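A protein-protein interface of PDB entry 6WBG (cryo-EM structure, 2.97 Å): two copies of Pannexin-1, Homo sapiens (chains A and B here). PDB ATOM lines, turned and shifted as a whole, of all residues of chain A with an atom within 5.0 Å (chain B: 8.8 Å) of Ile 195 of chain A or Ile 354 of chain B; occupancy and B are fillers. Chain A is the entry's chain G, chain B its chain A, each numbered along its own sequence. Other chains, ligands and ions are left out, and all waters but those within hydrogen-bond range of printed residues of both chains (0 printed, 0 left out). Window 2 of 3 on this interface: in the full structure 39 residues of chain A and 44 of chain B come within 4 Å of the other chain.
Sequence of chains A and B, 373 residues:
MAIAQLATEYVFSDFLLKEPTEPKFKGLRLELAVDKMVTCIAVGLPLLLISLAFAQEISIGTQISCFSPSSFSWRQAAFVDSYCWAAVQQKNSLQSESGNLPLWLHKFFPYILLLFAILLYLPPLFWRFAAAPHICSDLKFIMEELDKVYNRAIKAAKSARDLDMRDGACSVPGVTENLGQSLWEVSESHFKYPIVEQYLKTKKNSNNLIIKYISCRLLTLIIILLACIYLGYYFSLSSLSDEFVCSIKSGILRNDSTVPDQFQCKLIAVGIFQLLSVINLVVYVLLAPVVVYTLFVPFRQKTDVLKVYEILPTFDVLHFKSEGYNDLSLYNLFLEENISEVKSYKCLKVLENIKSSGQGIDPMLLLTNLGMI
The side-chain hydroxyl (OH) of Tyr 199 of chain A lies within hydrogen-bond range of the side-chain amino group (NZ) of Lys 346 of chain B, at 3.5 Å.
O of Asn 353 of chain B lies within hydrogen-bond range of OG1 of Thr 202 of chain A (3.4 Å).
The side-chain carboxylate (OE1) of Glu 352 of chain B sits close to the side-chain amide oxygen (OD1) of Asn 353 of chain B, 3.3 Å away.
The backbone carbonyl oxygen (O) of Gln 198 of chain A is in hydrogen-bond range of the side-chain hydroxyl (OG1) of Thr 202 of chain A (3.0 Å).
Among the printed residues, pairs that only touch across the chains: Phe 141 of chain A with Lys 346 of chain B, Phe 141 of chain A with Val 350 of chain B, Tyr 193 of chain A with Gln 359 of chain B, Tyr 193 of chain A with Gly 360 of chain B, Ile 195 of chain A with Ile 354 of chain B, Tyr 199 of chain A with Asn 353 of chain B and Thr 202 of chain A with Ile 354 of chain B.
Printed residues of chain A that touch a printed residue of chain B: Phe 141, Tyr 193, Ile 195, Tyr 199 and Thr 202.
Hydrophobic or aromatic side chains of chain B within 4 Å of the printed part of chain A: Val 350 and Ile 354.
Among the printed residues, 9 pairs touch across the chains.
Among the printed residues, no Asp or Glu carboxylate lies within 4 Å of a Lys or Arg side-chain nitrogen of the other chain.
No position is printed for both chains.
Of the 9 pairs that touch across the chains among the printed residues, none has its exchanged pair printed and touching as well.
Ile 195 of chain A touches one residue of chain B.
Printed residues of chain A within 4 Å of Ile 354 of chain B: Ile 195 and Thr 202.
No residue of chain B comes within 4 Å of Pro 194 of chain A.
Printed residues of chain B within 4 Å of Tyr 199 of chain A: Lys 346 and Asn 353.
Of the printed residues of chain A, Gln 359 of chain B touches Tyr 193.
Printed residues of chain B within 4 Å of Tyr 193 of chain A: Gln 359 (3.7 Å) and Gly 360 (3.6 Å).
Of the printed residues of chain B, Thr 202 of chain A touches Asn 353 and Ile 354.
The nearest printed residue of chain A that does not touch Ile 354 of chain B is Gln 198 of chain A (4.01 Å).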
ATOM      1  N   PHE A 141      24.083   6.211 -20.328  1.00  0.00           N
ATOM      2  CA  PHE A 141      23.261   5.057 -20.667  1.00  0.00           C
ATOM      3  C   PHE A 141      21.836   5.473 -21.003  1.00  0.00           C
ATOM      4  O   PHE A 141      21.236   4.935 -21.938  1.00  0.00           O
ATOM      5  CB  PHE A 141      23.261   4.053 -19.519  1.00  0.00           C
ATOM      6  CG  PHE A 141      22.186   3.018 -19.631  1.00  0.00           C
ATOM      7  CD1 PHE A 141      22.338   1.936 -20.475  1.00  0.00           C
ATOM      8  CD2 PHE A 141      21.017   3.133 -18.900  1.00  0.00           C
ATOM      9  CE1 PHE A 141      21.349   0.984 -20.585  1.00  0.00           C
ATOM     10  CE2 PHE A 141      20.024   2.185 -19.009  1.00  0.00           C
ATOM     11  CZ  PHE A 141      20.191   1.110 -19.852  1.00  0.00           C
ATOM     12  N   GLU A 145      20.011   4.865 -24.547  1.00  0.00           N
ATOM     13  CA  GLU A 145      18.759   4.123 -24.624  1.00  0.00           C
ATOM     14  C   GLU A 145      17.662   4.957 -25.267  1.00  0.00           C
ATOM     15  O   GLU A 145      16.822   4.426 -26.002  1.00  0.00           O
ATOM     16  CB  GLU A 145      18.335   3.664 -23.230  1.00  0.00           C
ATOM     17  N   TYR A 193      10.423  -3.586 -24.469  1.00  0.00           N
ATOM     18  CA  TYR A 193      10.458  -3.412 -23.024  1.00  0.00           C
ATOM     19  C   TYR A 193      10.891  -1.993 -22.690  1.00  0.00           C
ATOM     20  O   TYR A 193      11.944  -1.542 -23.173  1.00  0.00           O
ATOM     21  CB  TYR A 193      11.406  -4.421 -22.373  1.00  0.00           C
ATOM     22  CG  TYR A 193      11.178  -4.589 -20.887  1.00  0.00           C
ATOM     23  CD1 TYR A 193      11.837  -3.781 -19.971  1.00  0.00           C
ATOM     24  CD2 TYR A 193      10.299  -5.546 -20.404  1.00  0.00           C
ATOM     25  CE1 TYR A 193      11.633  -3.927 -18.614  1.00  0.00           C
ATOM     26  CE2 TYR A 193      10.086  -5.699 -19.049  1.00  0.00           C
ATOM     27  CZ  TYR A 193      10.755  -4.887 -18.159  1.00  0.00           C
ATOM     28  OH  TYR A 193      10.546  -5.036 -16.807  1.00  0.00           O
ATOM     29  N   PRO A 194      10.133  -1.252 -21.884  1.00  0.00           N
ATOM     30  CA  PRO A 194      10.574   0.090 -21.486  1.00  0.00           C
ATOM     31  C   PRO A 194      11.718   0.021 -20.489  1.00  0.00           C
ATOM     32  O   PRO A 194      11.512   0.175 -19.282  1.00  0.00           O
ATOM     33  CB  PRO A 194       9.316   0.703 -20.867  1.00  0.00           C
ATOM     34  CG  PRO A 194       8.550  -0.467 -20.353  1.00  0.00           C
ATOM     35  CD  PRO A 194       8.835  -1.612 -21.290  1.00  0.00           C
ATOM     36  N   ILE A 195      12.931  -0.216 -20.988  1.00  0.00           N
ATOM     37  CA  ILE A 195      14.065  -0.432 -20.097  1.00  0.00           C
ATOM     38  C   ILE A 195      14.468   0.865 -19.407  1.00  0.00           C
ATOM     39  O   ILE A 195      14.765   0.877 -18.208  1.00  0.00           O
ATOM     40  CB  ILE A 195      15.239  -1.065 -20.867  1.00  0.00           C
ATOM     41  CG1 ILE A 195      16.441  -1.258 -19.942  1.00  0.00           C
ATOM     42  CG2 ILE A 195      15.607  -0.233 -22.087  1.00  0.00           C
ATOM     43  CD1 ILE A 195      17.524  -2.124 -20.533  1.00  0.00           C
ATOM     44  N   VAL A 196      14.477   1.980 -20.142  1.00  0.00           N
ATOM     45  CA  VAL A 196      14.888   3.245 -19.543  1.00  0.00           C
ATOM     46  C   VAL A 196      13.834   3.728 -18.555  1.00  0.00           C
ATOM     47  O   VAL A 196      14.157   4.303 -17.507  1.00  0.00           O
ATOM     48  CB  VAL A 196      15.186   4.287 -20.636  1.00  0.00           C
ATOM     49  CG1 VAL A 196      13.923   4.676 -21.384  1.00  0.00           C
ATOM     50  CG2 VAL A 196      15.847   5.510 -20.031  1.00  0.00           C
ATOM     51  N   GLU A 197      12.558   3.476 -18.853  1.00  0.00           N
ATOM     52  CA  GLU A 197      11.503   3.838 -17.917  1.00  0.00           C
ATOM     53  C   GLU A 197      11.626   3.040 -16.627  1.00  0.00           C
ATOM     54  O   GLU A 197      11.460   3.586 -15.531  1.00  0.00           O
ATOM     55  CB  GLU A 197      10.136   3.623 -18.563  1.00  0.00           C
ATOM     56  CG  GLU A 197       8.982   4.257 -17.812  1.00  0.00           C
ATOM     57  CD  GLU A 197       8.330   3.302 -16.833  1.00  0.00           C
ATOM     58  OE1 GLU A 197       8.384   2.079 -17.073  1.00  0.00           O
ATOM     59  OE2 GLU A 197       7.760   3.776 -15.827  1.00  0.00           O
ATOM     60  N   GLN A 198      11.938   1.746 -16.734  1.00  0.00           N
ATOM     61  CA  GLN A 198      12.129   0.937 -15.537  1.00  0.00           C
ATOM     62  C   GLN A 198      13.365   1.379 -14.767  1.00  0.00           C
ATOM     63  O   GLN A 198      13.366   1.381 -13.529  1.00  0.00           O
ATOM     64  CB  GLN A 198      12.228  -0.539 -15.914  1.00  0.00           C
ATOM     65  CG  GLN A 198      10.885  -1.211 -16.126  1.00  0.00           C
ATOM     66  CD  GLN A 198      10.003  -1.149 -14.895  1.00  0.00           C
ATOM     67  OE1 GLN A 198       8.834  -0.776 -14.976  1.00  0.00           O
ATOM     68  NE2 GLN A 198      10.562  -1.514 -13.747  1.00  0.00           N
ATOM     69  N   TYR A 199      14.422   1.772 -15.477  1.00  0.00           N
ATOM     70  CA  TYR A 199      15.624   2.256 -14.807  1.00  0.00           C
ATOM     71  C   TYR A 199      15.333   3.520 -14.011  1.00  0.00           C
ATOM     72  O   TYR A 199      15.787   3.674 -12.872  1.00  0.00           O
ATOM     73  CB  TYR A 199      16.727   2.512 -15.832  1.00  0.00           C
ATOM     74  CG  TYR A 199      18.081   2.690 -15.206  1.00  0.00           C
ATOM     75  CD1 TYR A 199      18.409   2.036 -14.029  1.00  0.00           C
ATOM     76  CD2 TYR A 199      19.033   3.516 -15.782  1.00  0.00           C
ATOM     77  CE1 TYR A 199      19.643   2.190 -13.448  1.00  0.00           C
ATOM     78  CE2 TYR A 199      20.274   3.678 -15.206  1.00  0.00           C
ATOM     79  CZ  TYR A 199      20.571   3.012 -14.039  1.00  0.00           C
ATOM     80  OH  TYR A 199      21.806   3.166 -13.454  1.00  0.00           O
ATOM     81  N   THR A 202      13.464   2.780 -10.976  1.00  0.00           N
ATOM     82  CA  THR A 202      14.372   2.311  -9.933  1.00  0.00           C
ATOM     83  C   THR A 202      15.091   3.477  -9.270  1.00  0.00           C
ATOM     84  O   THR A 202      15.220   3.516  -8.038  1.00  0.00           O
ATOM     85  CB  THR A 202      15.378   1.327 -10.522  1.00  0.00           C
ATOM     86  OG1 THR A 202      14.680   0.203 -11.067  1.00  0.00           O
ATOM     87  CG2 THR A 202      16.333   0.845  -9.440  1.00  0.00           C
ATOM     88  N   TYR B 150      30.328 -11.560 -21.515  1.00  0.00           N
ATOM     89  CA  TYR B 150      29.036 -10.911 -21.728  1.00  0.00           C
ATOM     90  C   TYR B 150      28.592 -11.039 -23.181  1.00  0.00           C
ATOM     91  O   TYR B 150      27.435 -11.378 -23.465  1.00  0.00           O
ATOM     92  CB  TYR B 150      29.126  -9.444 -21.318  1.00  0.00           C
ATOM     93  CG  TYR B 150      27.844  -8.662 -21.475  1.00  0.00           C
ATOM     94  CD1 TYR B 150      26.808  -8.801 -20.563  1.00  0.00           C
ATOM     95  CD2 TYR B 150      27.677  -7.774 -22.525  1.00  0.00           C
ATOM     96  CE1 TYR B 150      25.643  -8.081 -20.699  1.00  0.00           C
ATOM     97  CE2 TYR B 150      26.516  -7.053 -22.669  1.00  0.00           C
ATOM     98  CZ  TYR B 150      25.502  -7.208 -21.754  1.00  0.00           C
ATOM     99  OH  TYR B 150      24.342  -6.489 -21.896  1.00  0.00           O
ATOM    100  N   LYS B 346      28.088  -2.063 -16.849  1.00  0.00           N
ATOM    101  CA  LYS B 346      27.066  -1.028 -16.754  1.00  0.00           C
ATOM    102  C   LYS B 346      25.695  -1.579 -17.121  1.00  0.00           C
ATOM    103  O   LYS B 346      24.721  -1.381 -16.386  1.00  0.00           O
ATOM    104  CB  LYS B 346      27.428   0.153 -17.648  1.00  0.00           C
ATOM    105  CG  LYS B 346      26.459   1.307 -17.524  1.00  0.00           C
ATOM    106  CD  LYS B 346      26.407   1.790 -16.088  1.00  0.00           C
ATOM    107  CE  LYS B 346      25.404   2.909 -15.915  1.00  0.00           C
ATOM    108  NZ  LYS B 346      24.007   2.429 -16.024  1.00  0.00           N
ATOM    109  N   CYS B 347      25.606  -2.284 -18.250  1.00  0.00           N
ATOM    110  CA  CYS B 347      24.319  -2.842 -18.655  1.00  0.00           C
ATOM    111  C   CYS B 347      23.825  -3.887 -17.665  1.00  0.00           C
ATOM    112  O   CYS B 347      22.631  -3.929 -17.342  1.00  0.00           O
ATOM    113  CB  CYS B 347      24.425  -3.444 -20.054  1.00  0.00           C
ATOM    114  SG  CYS B 347      25.253  -2.387 -21.256  1.00  0.00           S
ATOM    115  N   LEU B 348      24.727  -4.732 -17.165  1.00  0.00           N
ATOM    116  CA  LEU B 348      24.316  -5.738 -16.197  1.00  0.00           C
ATOM    117  C   LEU B 348      23.810  -5.093 -14.919  1.00  0.00           C
ATOM    118  O   LEU B 348      22.857  -5.585 -14.307  1.00  0.00           O
ATOM    119  CB  LEU B 348      25.474  -6.684 -15.904  1.00  0.00           C
ATOM    120  CG  LEU B 348      25.639  -7.793 -16.940  1.00  0.00           C
ATOM    121  CD1 LEU B 348      26.895  -8.595 -16.672  1.00  0.00           C
ATOM    122  CD2 LEU B 348      24.416  -8.690 -16.928  1.00  0.00           C
ATOM    123  N   LYS B 349      24.421  -3.983 -14.503  1.00  0.00           N
ATOM    124  CA  LYS B 349      23.947  -3.302 -13.305  1.00  0.00           C
ATOM    125  C   LYS B 349      22.603  -2.638 -13.555  1.00  0.00           C
ATOM    126  O   LYS B 349      21.758  -2.576 -12.656  1.00  0.00           O
ATOM    127  CB  LYS B 349      24.980  -2.283 -12.829  1.00  0.00           C
ATOM    128  CG  LYS B 349      24.501  -1.422 -11.674  1.00  0.00           C
ATOM    129  CD  LYS B 349      25.622  -1.134 -10.696  1.00  0.00           C
ATOM    130  CE  LYS B 349      25.768  -2.268  -9.697  1.00  0.00           C
ATOM    131  NZ  LYS B 349      24.578  -2.390  -8.812  1.00  0.00           N
ATOM    132  N   VAL B 350      22.386  -2.137 -14.773  1.00  0.00           N
ATOM    133  CA  VAL B 350      21.051  -1.674 -15.134  1.00  0.00           C
ATOM    134  C   VAL B 350      20.024  -2.775 -14.958  1.00  0.00           C
ATOM    135  O   VAL B 350      18.986  -2.558 -14.323  1.00  0.00           O
ATOM    136  CB  VAL B 350      21.006  -1.146 -16.578  1.00  0.00           C
ATOM    137  CG1 VAL B 350      19.603  -0.695 -16.905  1.00  0.00           C
ATOM    138  CG2 VAL B 350      21.966   0.001 -16.750  1.00  0.00           C
ATOM    139  N   LEU B 351      20.289  -3.962 -15.504  1.00  0.00           N
ATOM    140  CA  LEU B 351      19.348  -5.065 -15.327  1.00  0.00           C
ATOM    141  C   LEU B 351      19.188  -5.451 -13.860  1.00  0.00           C
ATOM    142  O   LEU B 351      18.081  -5.764 -13.415  1.00  0.00           O
ATOM    143  CB  LEU B 351      19.774  -6.281 -16.149  1.00  0.00           C
ATOM    144  CG  LEU B 351      19.395  -6.320 -17.632  1.00  0.00           C
ATOM    145  CD1 LEU B 351      20.192  -5.352 -18.480  1.00  0.00           C
ATOM    146  CD2 LEU B 351      19.558  -7.735 -18.151  1.00  0.00           C
ATOM    147  N   GLU B 352      20.277  -5.424 -13.093  1.00  0.00           N
ATOM    148  CA  GLU B 352      20.203  -5.822 -11.693  1.00  0.00           C
ATOM    149  C   GLU B 352      19.356  -4.847 -10.889  1.00  0.00           C
ATOM    150  O   GLU B 352      18.589  -5.257 -10.009  1.00  0.00           O
ATOM    151  CB  GLU B 352      21.611  -5.929 -11.109  1.00  0.00           C
ATOM    152  CG  GLU B 352      21.696  -6.747  -9.835  1.00  0.00           C
ATOM    153  CD  GLU B 352      21.489  -5.907  -8.592  1.00  0.00           C
ATOM    154  OE1 GLU B 352      21.800  -4.699  -8.636  1.00  0.00           O
ATOM    155  OE2 GLU B 352      21.019  -6.453  -7.574  1.00  0.00           O
ATOM    156  N   ASN B 353      19.480  -3.550 -11.174  1.00  0.00           N
ATOM    157  CA  ASN B 353      18.672  -2.553 -10.482  1.00  0.00           C
ATOM    158  C   ASN B 353      17.203  -2.695 -10.850  1.00  0.00           C
ATOM    159  O   ASN B 353      16.319  -2.554  -9.998  1.00  0.00           O
ATOM    160  CB  ASN B 353      19.181  -1.151 -10.810  1.00  0.00           C
ATOM    161  CG  ASN B 353      20.426  -0.788 -10.033  1.00  0.00           C
ATOM    162  OD1 ASN B 353      20.926  -1.582  -9.237  1.00  0.00           O
ATOM    163  ND2 ASN B 353      20.936   0.416 -10.260  1.00  0.00           N
ATOM    164  N   ILE B 354      16.922  -2.962 -12.126  1.00  0.00           N
ATOM    165  CA  ILE B 354      15.548  -3.205 -12.548  1.00  0.00           C
ATOM    166  C   ILE B 354      14.986  -4.426 -11.833  1.00  0.00           C
ATOM    167  O   ILE B 354      13.804  -4.463 -11.464  1.00  0.00           O
ATOM    168  CB  ILE B 354      15.480  -3.360 -14.077  1.00  0.00           C
ATOM    169  CG1 ILE B 354      15.850  -2.043 -14.759  1.00  0.00           C
ATOM    170  CG2 ILE B 354      14.099  -3.802 -14.513  1.00  0.00           C
ATOM    171  CD1 ILE B 354      16.026  -2.167 -16.249  1.00  0.00           C
ATOM    172  N   LYS B 355      15.827  -5.435 -11.608  1.00  0.00           N
ATOM    173  CA  LYS B 355      15.403  -6.659 -10.942  1.00  0.00           C
ATOM    174  C   LYS B 355      14.921  -6.407  -9.518  1.00  0.00           C
ATOM    175  O   LYS B 355      14.264  -7.265  -8.926  1.00  0.00           O
ATOM    176  CB  LYS B 355      16.540  -7.682 -10.935  1.00  0.00           C
ATOM    177  CG  LYS B 355      16.611  -8.534 -12.188  1.00  0.00           C
ATOM    178  CD  LYS B 355      15.278  -9.202 -12.471  1.00  0.00           C
ATOM    179  CE  LYS B 355      14.937 -10.230 -11.404  1.00  0.00           C
ATOM    180  NZ  LYS B 355      16.001 -11.259 -11.262  1.00  0.00           N
ATOM    181  N   SER B 356      15.257  -5.244  -8.955  1.00  0.00           N
ATOM    182  CA  SER B 356      14.751  -4.896  -7.630  1.00  0.00           C
ATOM    183  C   SER B 356      13.230  -4.844  -7.627  1.00  0.00           C
ATOM    184  O   SER B 356      12.581  -5.292  -6.674  1.00  0.00           O
ATOM    185  CB  SER B 356      15.339  -3.562  -7.173  1.00  0.00           C
ATOM    186  N   SER B 357      12.639  -4.297  -8.690  1.00  0.00           N
ATOM    187  CA  SER B 357      11.186  -4.330  -8.827  1.00  0.00           C
ATOM    188  C   SER B 357      10.706  -5.739  -9.144  1.00  0.00           C
ATOM    189  O   SER B 357       9.644  -6.165  -8.675  1.00  0.00           O
ATOM    190  CB  SER B 357      10.739  -3.348  -9.908  1.00  0.00           C
ATOM    191  N   GLY B 358      11.473  -6.480  -9.940  1.00  0.00           N
ATOM    192  CA  GLY B 358      11.121  -7.836 -10.298  1.00  0.00           C
ATOM    193  C   GLY B 358      10.009  -7.964 -11.316  1.00  0.00           C
ATOM    194  O   GLY B 358       9.325  -8.994 -11.327  1.00  0.00           O
ATOM    195  N   GLN B 359       9.803  -6.955 -12.164  1.00  0.00           N
ATOM    196  CA  GLN B 359       8.694  -7.000 -13.111  1.00  0.00           C
ATOM    197  C   GLN B 359       8.896  -8.087 -14.159  1.00  0.00           C
ATOM    198  O   GLN B 359       8.080  -9.009 -14.268  1.00  0.00           O
ATOM    199  CB  GLN B 359       8.523  -5.635 -13.779  1.00  0.00           C
ATOM    200  N   GLY B 360       9.977  -8.000 -14.936  1.00  0.00           N
ATOM    201  CA  GLY B 360      10.163  -8.944 -16.027  1.00  0.00           C
ATOM    202  C   GLY B 360      11.080 -10.096 -15.664  1.00  0.00           C
ATOM    203  O   GLY B 360      10.835 -10.819 -14.695  1.00  0.00           O
ATOM    204  N   ILE B 361      12.150 -10.279 -16.434  1.00  0.00           N
ATOM    205  CA  ILE B 361      13.075 -11.391 -16.235  1.00  0.00           C
ATOM    206  C   ILE B 361      14.447 -10.993 -16.757  1.00  0.00           C
ATOM    207  O   ILE B 361      14.561 -10.169 -17.670  1.00  0.00           O
ATOM    208  CB  ILE B 361      12.569 -12.670 -16.925  1.00  0.00           C
ATOM    209  N   ASP B 362      15.494 -11.577 -16.183  1.00  0.00           N
ATOM    210  CA  ASP B 362      16.866 -11.217 -16.517  1.00  0.00           C
ATOM    211  C   ASP B 362      17.227 -11.568 -17.961  1.00  0.00           C
ATOM    212  O   ASP B 362      17.713 -10.693 -18.690  1.00  0.00           O
ATOM    213  CB  ASP B 362      17.844 -11.883 -15.545  1.00  0.00           C
ATOM    214  N   MET B 364      15.349 -12.155 -20.614  1.00  0.00           N
ATOM    215  CA  MET B 364      14.542 -11.404 -21.570  1.00  0.00           C
ATOM    216  C   MET B 364      15.035  -9.970 -21.699  1.00  0.00           C
ATOM    217  O   MET B 364      15.226  -9.467 -22.812  1.00  0.00           O
ATOM    218  CB  MET B 364      13.072 -11.432 -21.149  1.00  0.00           C
ATOM    219  N   LEU B 365      15.254  -9.297 -20.566  1.00  0.00           N
ATOM    220  CA  LEU B 365      15.751  -7.926 -20.609  1.00  0.00           C
ATOM    221  C   LEU B 365      17.154  -7.868 -21.198  1.00  0.00           C
ATOM    222  O   LEU B 365      17.512  -6.892 -21.868  1.00  0.00           O
ATOM    223  CB  LEU B 365      15.730  -7.316 -19.207  1.00  0.00           C
ATOM    224  N   LEU B 366      17.960  -8.905 -20.965  1.00  0.00           N
ATOM    225  CA  LEU B 366      19.292  -8.944 -21.560  1.00  0.00           C
ATOM    226  C   LEU B 366      19.212  -9.044 -23.076  1.00  0.00           C
ATOM    227  O   LEU B 366      19.905  -8.312 -23.793  1.00  0.00           O
ATOM    228  CB  LEU B 366      20.090 -10.116 -20.986  1.00  0.00           C
ATOM    229  N   LEU B 367      18.369  -9.946 -23.582  1.00  0.00           N
ATOM    230  CA  LEU B 367      18.168 -10.046 -25.022  1.00  0.00           C
ATOM    231  C   LEU B 367      17.634  -8.739 -25.592  1.00  0.00           C
ATOM    232  O   LEU B 367      17.999  -8.343 -26.705  1.00  0.00           O
ATOM    233  CB  LEU B 367      17.217 -11.198 -25.341  1.00  0.00           C
ATOM    234  N   THR B 368      16.772  -8.054 -24.838  1.00  0.00           N
ATOM    235  CA  THR B 368      16.276  -6.754 -25.278  1.00  0.00           C
ATOM    236  C   THR B 368      17.406  -5.738 -25.366  1.00  0.00           C
ATOM    237  O   THR B 368      17.451  -4.930 -26.302  1.00  0.00           O
ATOM    238  CB  THR B 368      15.183  -6.259 -24.334  1.00  0.00           C
ATOM    239  N   ASN B 369      18.300  -5.788 -24.367  1.00  0.00           N
ATOM    240  CA  ASN B 369      19.475  -4.883 -24.197  1.00  0.00           C
ATOM    241  C   ASN B 369      20.135  -4.576 -25.545  1.00  0.00           C
ATOM    242  O   ASN B 369      20.060  -3.408 -25.982  1.00  0.00           O
ATOM    243  CB  ASN B 369      20.490  -5.458 -23.203  1.00  0.00           C
ATOM    244  N   LEU B 370      20.694  -5.618 -26.176  1.00  0.00           N
ATOM    245  CA  LEU B 370      21.395  -5.570 -27.492  1.00  0.00           C
ATOM    246  C   LEU B 370      22.581  -4.604 -27.424  1.00  0.00           C
ATOM    247  O   LEU B 370      22.624  -3.655 -28.231  1.00  0.00           O
ATOM    248  CB  LEU B 370      20.414  -5.207 -28.615  1.00  0.00           C
